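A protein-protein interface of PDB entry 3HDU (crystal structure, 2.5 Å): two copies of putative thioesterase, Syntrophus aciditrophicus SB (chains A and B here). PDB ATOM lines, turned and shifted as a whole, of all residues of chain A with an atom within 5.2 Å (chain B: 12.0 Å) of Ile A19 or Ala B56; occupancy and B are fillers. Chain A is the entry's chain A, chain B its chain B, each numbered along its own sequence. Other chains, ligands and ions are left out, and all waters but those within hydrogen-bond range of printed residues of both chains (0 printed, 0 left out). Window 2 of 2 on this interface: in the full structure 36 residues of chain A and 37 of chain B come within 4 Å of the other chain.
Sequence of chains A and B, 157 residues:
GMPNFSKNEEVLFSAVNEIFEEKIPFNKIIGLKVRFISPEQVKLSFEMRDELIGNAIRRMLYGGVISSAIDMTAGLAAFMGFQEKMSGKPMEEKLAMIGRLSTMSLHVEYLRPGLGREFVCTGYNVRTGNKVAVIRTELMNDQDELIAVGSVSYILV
Hydrophobic or aromatic side chains of chain A that line the printed part of chain B: Ile A19, Phe A20, Ile A24 and Ile A98.
Hydrophobic or aromatic side chains of chain B within 4 Å of the printed part of chain A: Ala B56, Ile B57, Met B60 and Leu B61.
Along chain B the printed residues that touch a printed residue of chain A span positions 55 to 61.
Among the printed residues, 10 pairs touch across the chains.
Among the printed residues, no Asp or Glu carboxylate lies within 4 Å of a Lys or Arg side-chain nitrogen of the other chain.
Ala A15 touches none of the printed residues of chain B.
No residue of chain B comes within 4 Å of Val A16.
No residue of chain B comes within 4 Å of Glu A18.
Ile A19 touches just these residues of chain B: Ala B56 (3.9 Å) and Ile B57 (3.7 Å).
No residue of chain B comes within 4 Å of Glu A22.
Of chain B, only Leu B61 comes within 4 Å of Ile A24.
Of chain B, only Ala B56 and Arg B59 come within 4 Å of Gly A99.
Gly B54 touches none of the printed residues of chain A.
Of the printed residues of chain A, Ala B56 touches Ile A19 (3.9 Å), Ile A98 (3.6 Å) and Gly A99 (3.2 Å).
Of the printed residues of chain A, Ile B57 touches Ile A19 (3.7 Å), Phe A20 (3.7 Å) and Ile A98 (3.7 Å).
Arg B58 touches none of the printed residues of chain A.
Of the printed residues of chain A, Arg B59 touches Gly A99.
Of the printed residues of chain A, Met B60 touches Phe A20 (3.8 Å).
Printed residues of chain A within 4 Å of Leu B61: Ile A24 (3.9 Å).
Among the printed residues, pairs that only touch across the chains: Ile A19 with Ala B56 (3.9 Å), Ile A19 with Ile B57 (3.7 Å), Phe A20 with Ile B57 (3.7 Å), Phe A20 with Met B60 (3.8 Å), Ile A24 with Leu B61 (3.9 Å), Ile A98 with Ala B56 (3.6 Å) and Ile A98 with Ile B57 (3.7 Å).
The side-chain amide nitrogen of Asn B55 sits at hydrogen-bond distance from the backbone carbonyl oxygen of Lys A23 (3.2 Å).
N of Gly A99 sits close to O of Ala B56 (3.4 Å).
NE of Arg B59 lies within hydrogen-bond range of O of Gly A99 (3.3 Å).
The backbone carbonyl oxygen (O) of Glu A18 lies within hydrogen-bond range of the backbone NH (N) of Lys A23 (3.0 Å).
The backbone NH (N) of Ile B57 lies within hydrogen-bond range of the side-chain amide oxygen (OD1) of Asn B55.
No position is printed for both chains.
Of the 10 pairs that touch across the chains among the printed residues, none has its exchanged pair printed and touching as well.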
ATOM      1  N   ALA A  15     -33.181  10.666   6.019  1.00  0.00           N
ATOM      2  CA  ALA A  15     -32.080  10.489   5.051  1.00  0.00           C
ATOM      3  C   ALA A  15     -31.345   9.176   5.291  1.00  0.00           C
ATOM      4  O   ALA A  15     -31.065   8.437   4.343  1.00  0.00           O
ATOM      5  CB  ALA A  15     -31.098  11.651   5.134  1.00  0.00           C
ATOM      6  N   VAL A  16     -31.049   8.902   6.566  1.00  0.00           N
ATOM      7  CA  VAL A  16     -30.383   7.670   6.992  1.00  0.00           C
ATOM      8  C   VAL A  16     -31.258   6.441   6.700  1.00  0.00           C
ATOM      9  O   VAL A  16     -30.769   5.480   6.108  1.00  0.00           O
ATOM     10  CB  VAL A  16     -29.960   7.736   8.504  1.00  0.00           C
ATOM     11  CG1 VAL A  16     -29.518   6.369   9.040  1.00  0.00           C
ATOM     12  CG2 VAL A  16     -28.852   8.765   8.689  1.00  0.00           C
ATOM     13  N   ASN A  17     -32.538   6.489   7.082  1.00  0.00           N
ATOM     14  CA  ASN A  17     -33.476   5.374   6.822  1.00  0.00           C
ATOM     15  C   ASN A  17     -33.520   4.957   5.345  1.00  0.00           C
ATOM     16  O   ASN A  17     -33.487   3.764   5.055  1.00  0.00           O
ATOM     17  CB  ASN A  17     -34.894   5.671   7.351  1.00  0.00           C
ATOM     18  CG  ASN A  17     -34.988   5.642   8.881  1.00  0.00           C
ATOM     19  OD1 ASN A  17     -34.005   5.422   9.592  1.00  0.00           O
ATOM     20  ND2 ASN A  17     -36.188   5.875   9.389  1.00  0.00           N
ATOM     21  N   GLU A  18     -33.556   5.937   4.436  1.00  0.00           N
ATOM     22  CA  GLU A  18     -33.511   5.672   2.977  1.00  0.00           C
ATOM     23  C   GLU A  18     -32.259   4.901   2.542  1.00  0.00           C
ATOM     24  O   GLU A  18     -32.366   3.877   1.866  1.00  0.00           O
ATOM     25  CB  GLU A  18     -33.617   6.971   2.146  1.00  0.00           C
ATOM     26  CG  GLU A  18     -35.028   7.331   1.685  1.00  0.00           C
ATOM     27  CD  GLU A  18     -35.495   6.537   0.454  1.00  0.00           C
ATOM     28  OE1 GLU A  18     -34.995   5.418   0.199  1.00  0.00           O
ATOM     29  OE2 GLU A  18     -36.374   7.042  -0.273  1.00  0.00           O
ATOM     30  N   ILE A  19     -31.095   5.395   2.963  1.00  0.00           N
ATOM     31  CA  ILE A  19     -29.789   4.816   2.603  1.00  0.00           C
ATOM     32  C   ILE A  19     -29.606   3.377   3.106  1.00  0.00           C
ATOM     33  O   ILE A  19     -29.181   2.513   2.337  1.00  0.00           O
ATOM     34  CB  ILE A  19     -28.607   5.721   3.099  1.00  0.00           C
ATOM     35  CG1 ILE A  19     -28.614   7.072   2.364  1.00  0.00           C
ATOM     36  CG2 ILE A  19     -27.243   5.048   2.874  1.00  0.00           C
ATOM     37  CD1 ILE A  19     -27.642   8.082   2.929  1.00  0.00           C
ATOM     38  N   PHE A  20     -29.956   3.130   4.369  1.00  0.00           N
ATOM     39  CA  PHE A  20     -29.790   1.806   5.007  1.00  0.00           C
ATOM     40  C   PHE A  20     -30.919   0.777   4.788  1.00  0.00           C
ATOM     41  O   PHE A  20     -30.626  -0.406   4.575  1.00  0.00           O
ATOM     42  CB  PHE A  20     -29.495   1.974   6.511  1.00  0.00           C
ATOM     43  CG  PHE A  20     -28.107   2.495   6.798  1.00  0.00           C
ATOM     44  CD1 PHE A  20     -27.835   3.867   6.788  1.00  0.00           C
ATOM     45  CD2 PHE A  20     -27.059   1.608   7.061  1.00  0.00           C
ATOM     46  CE1 PHE A  20     -26.543   4.353   7.047  1.00  0.00           C
ATOM     47  CE2 PHE A  20     -25.762   2.081   7.322  1.00  0.00           C
ATOM     48  CZ  PHE A  20     -25.504   3.458   7.314  1.00  0.00           C
ATOM     49  N   GLU A  21     -32.184   1.212   4.825  1.00  0.00           N
ATOM     50  CA  GLU A  21     -33.336   0.283   4.705  1.00  0.00           C
ATOM     51  C   GLU A  21     -33.777  -0.052   3.273  1.00  0.00           C
ATOM     52  O   GLU A  21     -34.076  -1.218   2.988  1.00  0.00           O
ATOM     53  CB  GLU A  21     -34.541   0.781   5.516  1.00  0.00           C
ATOM     54  CG  GLU A  21     -34.209   1.066   6.988  1.00  0.00           C
ATOM     55  CD  GLU A  21     -35.412   1.432   7.854  1.00  0.00           C
ATOM     56  OE1 GLU A  21     -36.575   1.293   7.413  1.00  0.00           O
ATOM     57  OE2 GLU A  21     -35.187   1.860   9.005  1.00  0.00           O
ATOM     58  N   GLU A  22     -33.822   0.951   2.390  1.00  0.00           N
ATOM     59  CA  GLU A  22     -34.268   0.772   0.987  1.00  0.00           C
ATOM     60  C   GLU A  22     -33.142   0.663  -0.056  1.00  0.00           C
ATOM     61  O   GLU A  22     -33.170  -0.244  -0.898  1.00  0.00           O
ATOM     62  CB  GLU A  22     -35.234   1.899   0.581  1.00  0.00           C
ATOM     63  CG  GLU A  22     -36.585   1.852   1.287  1.00  0.00           C
ATOM     64  N   LYS A  23     -32.161   1.567   0.009  1.00  0.00           N
ATOM     65  CA  LYS A  23     -31.091   1.656  -1.015  1.00  0.00           C
ATOM     66  C   LYS A  23     -30.021   0.547  -1.051  1.00  0.00           C
ATOM     67  O   LYS A  23     -29.366   0.398  -2.084  1.00  0.00           O
ATOM     68  CB  LYS A  23     -30.420   3.043  -0.986  1.00  0.00           C
ATOM     69  CG  LYS A  23     -31.342   4.232  -1.301  1.00  0.00           C
ATOM     70  CD  LYS A  23     -31.776   4.281  -2.756  1.00  0.00           C
ATOM     71  CE  LYS A  23     -32.599   5.525  -3.049  1.00  0.00           C
ATOM     72  NZ  LYS A  23     -33.061   5.568  -4.466  1.00  0.00           N
ATOM     73  N   ILE A  24     -29.835  -0.216   0.033  1.00  0.00           N
ATOM     74  CA  ILE A  24     -28.861  -1.334   0.053  1.00  0.00           C
ATOM     75  C   ILE A  24     -29.416  -2.489  -0.808  1.00  0.00           C
ATOM     76  O   ILE A  24     -30.550  -2.907  -0.575  1.00  0.00           O
ATOM     77  CB  ILE A  24     -28.591  -1.871   1.489  1.00  0.00           C
ATOM     78  CG1 ILE A  24     -27.958  -0.789   2.366  1.00  0.00           C
ATOM     79  CG2 ILE A  24     -27.664  -3.097   1.464  1.00  0.00           C
ATOM     80  CD1 ILE A  24     -27.632  -1.255   3.783  1.00  0.00           C
ATOM     81  N   ILE A  98     -21.066  10.817   4.360  1.00  0.00           N
ATOM     82  CA  ILE A  98     -21.264   9.368   4.600  1.00  0.00           C
ATOM     83  C   ILE A  98     -20.606   8.453   3.544  1.00  0.00           C
ATOM     84  O   ILE A  98     -20.234   7.323   3.858  1.00  0.00           O
ATOM     85  CB  ILE A  98     -22.774   8.994   4.795  1.00  0.00           C
ATOM     86  CG1 ILE A  98     -22.918   7.705   5.620  1.00  0.00           C
ATOM     87  CG2 ILE A  98     -23.508   8.907   3.453  1.00  0.00           C
ATOM     88  CD1 ILE A  98     -24.355   7.370   5.993  1.00  0.00           C
ATOM     89  N   GLY A  99     -20.465   8.952   2.316  1.00  0.00           N
ATOM     90  CA  GLY A  99     -19.773   8.239   1.241  1.00  0.00           C
ATOM     91  C   GLY A  99     -18.262   8.139   1.388  1.00  0.00           C
ATOM     92  O   GLY A  99     -17.645   7.325   0.701  1.00  0.00           O
ATOM     93  N   ASP B  50     -22.655  -7.197  -8.742  1.00  0.00           N
ATOM     94  CA  ASP B  50     -23.190  -5.839  -8.635  1.00  0.00           C
ATOM     95  C   ASP B  50     -22.070  -5.013  -7.984  1.00  0.00           C
ATOM     96  O   ASP B  50     -21.776  -5.195  -6.799  1.00  0.00           O
ATOM     97  CB  ASP B  50     -24.468  -5.825  -7.777  1.00  0.00           C
ATOM     98  CG  ASP B  50     -25.116  -4.435  -7.668  1.00  0.00           C
ATOM     99  OD1 ASP B  50     -24.848  -3.542  -8.499  1.00  0.00           O
ATOM    100  OD2 ASP B  50     -25.925  -4.246  -6.737  1.00  0.00           O
ATOM    101  N   GLU B  51     -21.443  -4.128  -8.764  1.00  0.00           N
ATOM    102  CA  GLU B  51     -20.327  -3.278  -8.270  1.00  0.00           C
ATOM    103  C   GLU B  51     -20.726  -2.099  -7.348  1.00  0.00           C
ATOM    104  O   GLU B  51     -19.839  -1.446  -6.784  1.00  0.00           O
ATOM    105  CB  GLU B  51     -19.440  -2.806  -9.439  1.00  0.00           C
ATOM    106  CG  GLU B  51     -18.479  -3.871  -9.956  1.00  0.00           C
ATOM    107  CD  GLU B  51     -17.758  -3.443 -11.223  1.00  0.00           C
ATOM    108  OE1 GLU B  51     -18.426  -3.308 -12.273  1.00  0.00           O
ATOM    109  OE2 GLU B  51     -16.519  -3.268 -11.176  1.00  0.00           O
ATOM    110  N   LEU B  52     -22.034  -1.839  -7.212  1.00  0.00           N
ATOM    111  CA  LEU B  52     -22.604  -0.830  -6.297  1.00  0.00           C
ATOM    112  C   LEU B  52     -22.244   0.631  -6.614  1.00  0.00           C
ATOM    113  O   LEU B  52     -22.162   1.459  -5.697  1.00  0.00           O
ATOM    114  CB  LEU B  52     -22.243  -1.163  -4.828  1.00  0.00           C
ATOM    115  CG  LEU B  52     -22.376  -2.602  -4.315  1.00  0.00           C
ATOM    116  CD1 LEU B  52     -21.869  -2.696  -2.885  1.00  0.00           C
ATOM    117  CD2 LEU B  52     -23.805  -3.079  -4.407  1.00  0.00           C
ATOM    118  N   ILE B  53     -22.079   0.957  -7.902  1.00  0.00           N
ATOM    119  CA  ILE B  53     -21.747   2.329  -8.331  1.00  0.00           C
ATOM    120  C   ILE B  53     -22.964   3.223  -8.069  1.00  0.00           C
ATOM    121  O   ILE B  53     -24.098   2.830  -8.362  1.00  0.00           O
ATOM    122  CB  ILE B  53     -21.336   2.439  -9.845  1.00  0.00           C
ATOM    123  CG1 ILE B  53     -20.018   1.705 -10.137  1.00  0.00           C
ATOM    124  CG2 ILE B  53     -21.189   3.911 -10.288  1.00  0.00           C
ATOM    125  CD1 ILE B  53     -20.171   0.246 -10.422  1.00  0.00           C
ATOM    126  N   GLY B  54     -22.714   4.406  -7.504  1.00  0.00           N
ATOM    127  CA  GLY B  54     -23.766   5.373  -7.179  1.00  0.00           C
ATOM    128  C   GLY B  54     -24.399   5.249  -5.799  1.00  0.00           C
ATOM    129  O   GLY B  54     -25.165   6.133  -5.412  1.00  0.00           O
ATOM    130  N   ASN B  55     -24.091   4.177  -5.059  1.00  0.00           N
ATOM    131  CA  ASN B  55     -24.636   3.964  -3.713  1.00  0.00           C
ATOM    132  C   ASN B  55     -23.941   4.912  -2.726  1.00  0.00           C
ATOM    133  O   ASN B  55     -22.716   5.069  -2.771  1.00  0.00           O
ATOM    134  CB  ASN B  55     -24.486   2.493  -3.290  1.00  0.00           C
ATOM    135  CG  ASN B  55     -25.242   2.158  -2.006  1.00  0.00           C
ATOM    136  OD1 ASN B  55     -24.880   2.608  -0.919  1.00  0.00           O
ATOM    137  ND2 ASN B  55     -26.275   1.328  -2.127  1.00  0.00           N
ATOM    138  N   ALA B  56     -24.734   5.520  -1.841  1.00  0.00           N
ATOM    139  CA  ALA B  56     -24.245   6.488  -0.844  1.00  0.00           C
ATOM    140  C   ALA B  56     -23.273   5.933   0.198  1.00  0.00           C
ATOM    141  O   ALA B  56     -22.511   6.704   0.767  1.00  0.00           O
ATOM    142  CB  ALA B  56     -25.417   7.163  -0.136  1.00  0.00           C
ATOM    143  N   ILE B  57     -23.324   4.623   0.465  1.00  0.00           N
ATOM    144  CA  ILE B  57     -22.427   3.950   1.427  1.00  0.00           C
ATOM    145  C   ILE B  57     -21.706   2.773   0.748  1.00  0.00           C
ATOM    146  O   ILE B  57     -21.574   1.689   1.317  1.00  0.00           O
ATOM    147  CB  ILE B  57     -23.179   3.537   2.740  1.00  0.00           C
ATOM    148  CG1 ILE B  57     -24.405   2.650   2.448  1.00  0.00           C
ATOM    149  CG2 ILE B  57     -23.593   4.780   3.512  1.00  0.00           C
ATOM    150  CD1 ILE B  57     -25.086   2.107   3.687  1.00  0.00           C
ATOM    151  N   ARG B  58     -21.204   3.028  -0.462  1.00  0.00           N
ATOM    152  CA  ARG B  58     -20.497   2.027  -1.277  1.00  0.00           C
ATOM    153  C   ARG B  58     -19.256   1.499  -0.553  1.00  0.00           C
ATOM    154  O   ARG B  58     -19.103   0.289  -0.403  1.00  0.00           O
ATOM    155  CB  ARG B  58     -20.104   2.628  -2.634  1.00  0.00           C
ATOM    156  CG  ARG B  58     -19.515   1.639  -3.626  1.00  0.00           C
ATOM    157  CD  ARG B  58     -19.025   2.339  -4.874  1.00  0.00           C
ATOM    158  NE  ARG B  58     -18.222   1.433  -5.698  1.00  0.00           N
ATOM    159  CZ  ARG B  58     -17.464   1.791  -6.738  1.00  0.00           C
ATOM    160  NH1 ARG B  58     -17.376   3.066  -7.140  1.00  0.00           N
ATOM    161  NH2 ARG B  58     -16.773   0.852  -7.391  1.00  0.00           N
ATOM    162  N   ARG B  59     -18.401   2.414  -0.093  1.00  0.00           N
ATOM    163  CA  ARG B  59     -17.164   2.060   0.651  1.00  0.00           C
ATOM    164  C   ARG B  59     -17.456   1.220   1.890  1.00  0.00           C
ATOM    165  O   ARG B  59     -16.738   0.263   2.182  1.00  0.00           O
ATOM    166  CB  ARG B  59     -16.383   3.308   1.095  1.00  0.00           C
ATOM    167  CG  ARG B  59     -15.858   4.176  -0.023  1.00  0.00           C
ATOM    168  CD  ARG B  59     -15.050   5.333   0.528  1.00  0.00           C
ATOM    169  NE  ARG B  59     -14.782   6.323  -0.517  1.00  0.00           N
ATOM    170  CZ  ARG B  59     -13.852   6.220  -1.473  1.00  0.00           C
ATOM    171  NH1 ARG B  59     -13.046   5.153  -1.566  1.00  0.00           N
ATOM    172  NH2 ARG B  59     -13.730   7.206  -2.370  1.00  0.00           N
ATOM    173  N   MET B  60     -18.519   1.594   2.598  1.00  0.00           N
ATOM    174  CA  MET B  60     -18.971   0.914   3.810  1.00  0.00           C
ATOM    175  C   MET B  60     -19.413  -0.517   3.499  1.00  0.00           C
ATOM    176  O   MET B  60     -18.968  -1.447   4.168  1.00  0.00           O
ATOM    177  CB  MET B  60     -20.117   1.708   4.436  1.00  0.00           C
ATOM    178  CG  MET B  60     -20.507   1.312   5.828  1.00  0.00           C
ATOM    179  SD  MET B  60     -21.896   2.482   6.479  1.00  0.00           S
ATOM    180  CE  MET B  60     -20.911   4.133   6.593  1.00  0.00           C
ATOM    181  N   LEU B  61     -20.267  -0.674   2.481  1.00  0.00           N
ATOM    182  CA  LEU B  61     -20.756  -1.993   2.022  1.00  0.00           C
ATOM    183  C   LEU B  61     -19.623  -2.935   1.592  1.00  0.00           C
ATOM    184  O   LEU B  61     -19.691  -4.135   1.863  1.00  0.00           O
ATOM    185  CB  LEU B  61     -21.792  -1.849   0.895  1.00  0.00           C
ATOM    186  CG  LEU B  61     -23.168  -1.282   1.277  1.00  0.00           C
ATOM    187  CD1 LEU B  61     -23.982  -0.952   0.034  1.00  0.00           C
ATOM    188  CD2 LEU B  61     -23.935  -2.236   2.186  1.00  0.00           C
ATOM    189  N   TYR B  62     -18.601  -2.384   0.931  1.00  0.00           N
ATOM    190  CA  TYR B  62     -17.391  -3.144   0.553  1.00  0.00           C
ATOM    191  C   TYR B  62     -16.610  -3.672   1.777  1.00  0.00           C
ATOM    192  O   TYR B  62     -15.960  -4.712   1.678  1.00  0.00           O
ATOM    193  CB  TYR B  62     -16.460  -2.340  -0.387  1.00  0.00           C
ATOM    194  CG  TYR B  62     -16.691  -2.570  -1.873  1.00  0.00           C
ATOM    195  CD1 TYR B  62     -17.647  -1.839  -2.590  1.00  0.00           C
ATOM    196  CD2 TYR B  62     -15.933  -3.522  -2.574  1.00  0.00           C
ATOM    197  CE1 TYR B  62     -17.850  -2.052  -3.976  1.00  0.00           C
ATOM    198  CE2 TYR B  62     -16.130  -3.747  -3.963  1.00  0.00           C
ATOM    199  CZ  TYR B  62     -17.085  -3.008  -4.652  1.00  0.00           C
ATOM    200  OH  TYR B  62     -17.276  -3.227  -6.000  1.00  0.00           O
ATOM    201  N   GLY B  63     -16.675  -2.960   2.907  1.00  0.00           N
ATOM    202  CA  GLY B  63     -16.040  -3.389   4.159  1.00  0.00           C
ATOM    203  C   GLY B  63     -16.580  -4.723   4.649  1.00  0.00           C
ATOM    204  O   GLY B  63     -15.805  -5.619   5.011  1.00  0.00           O
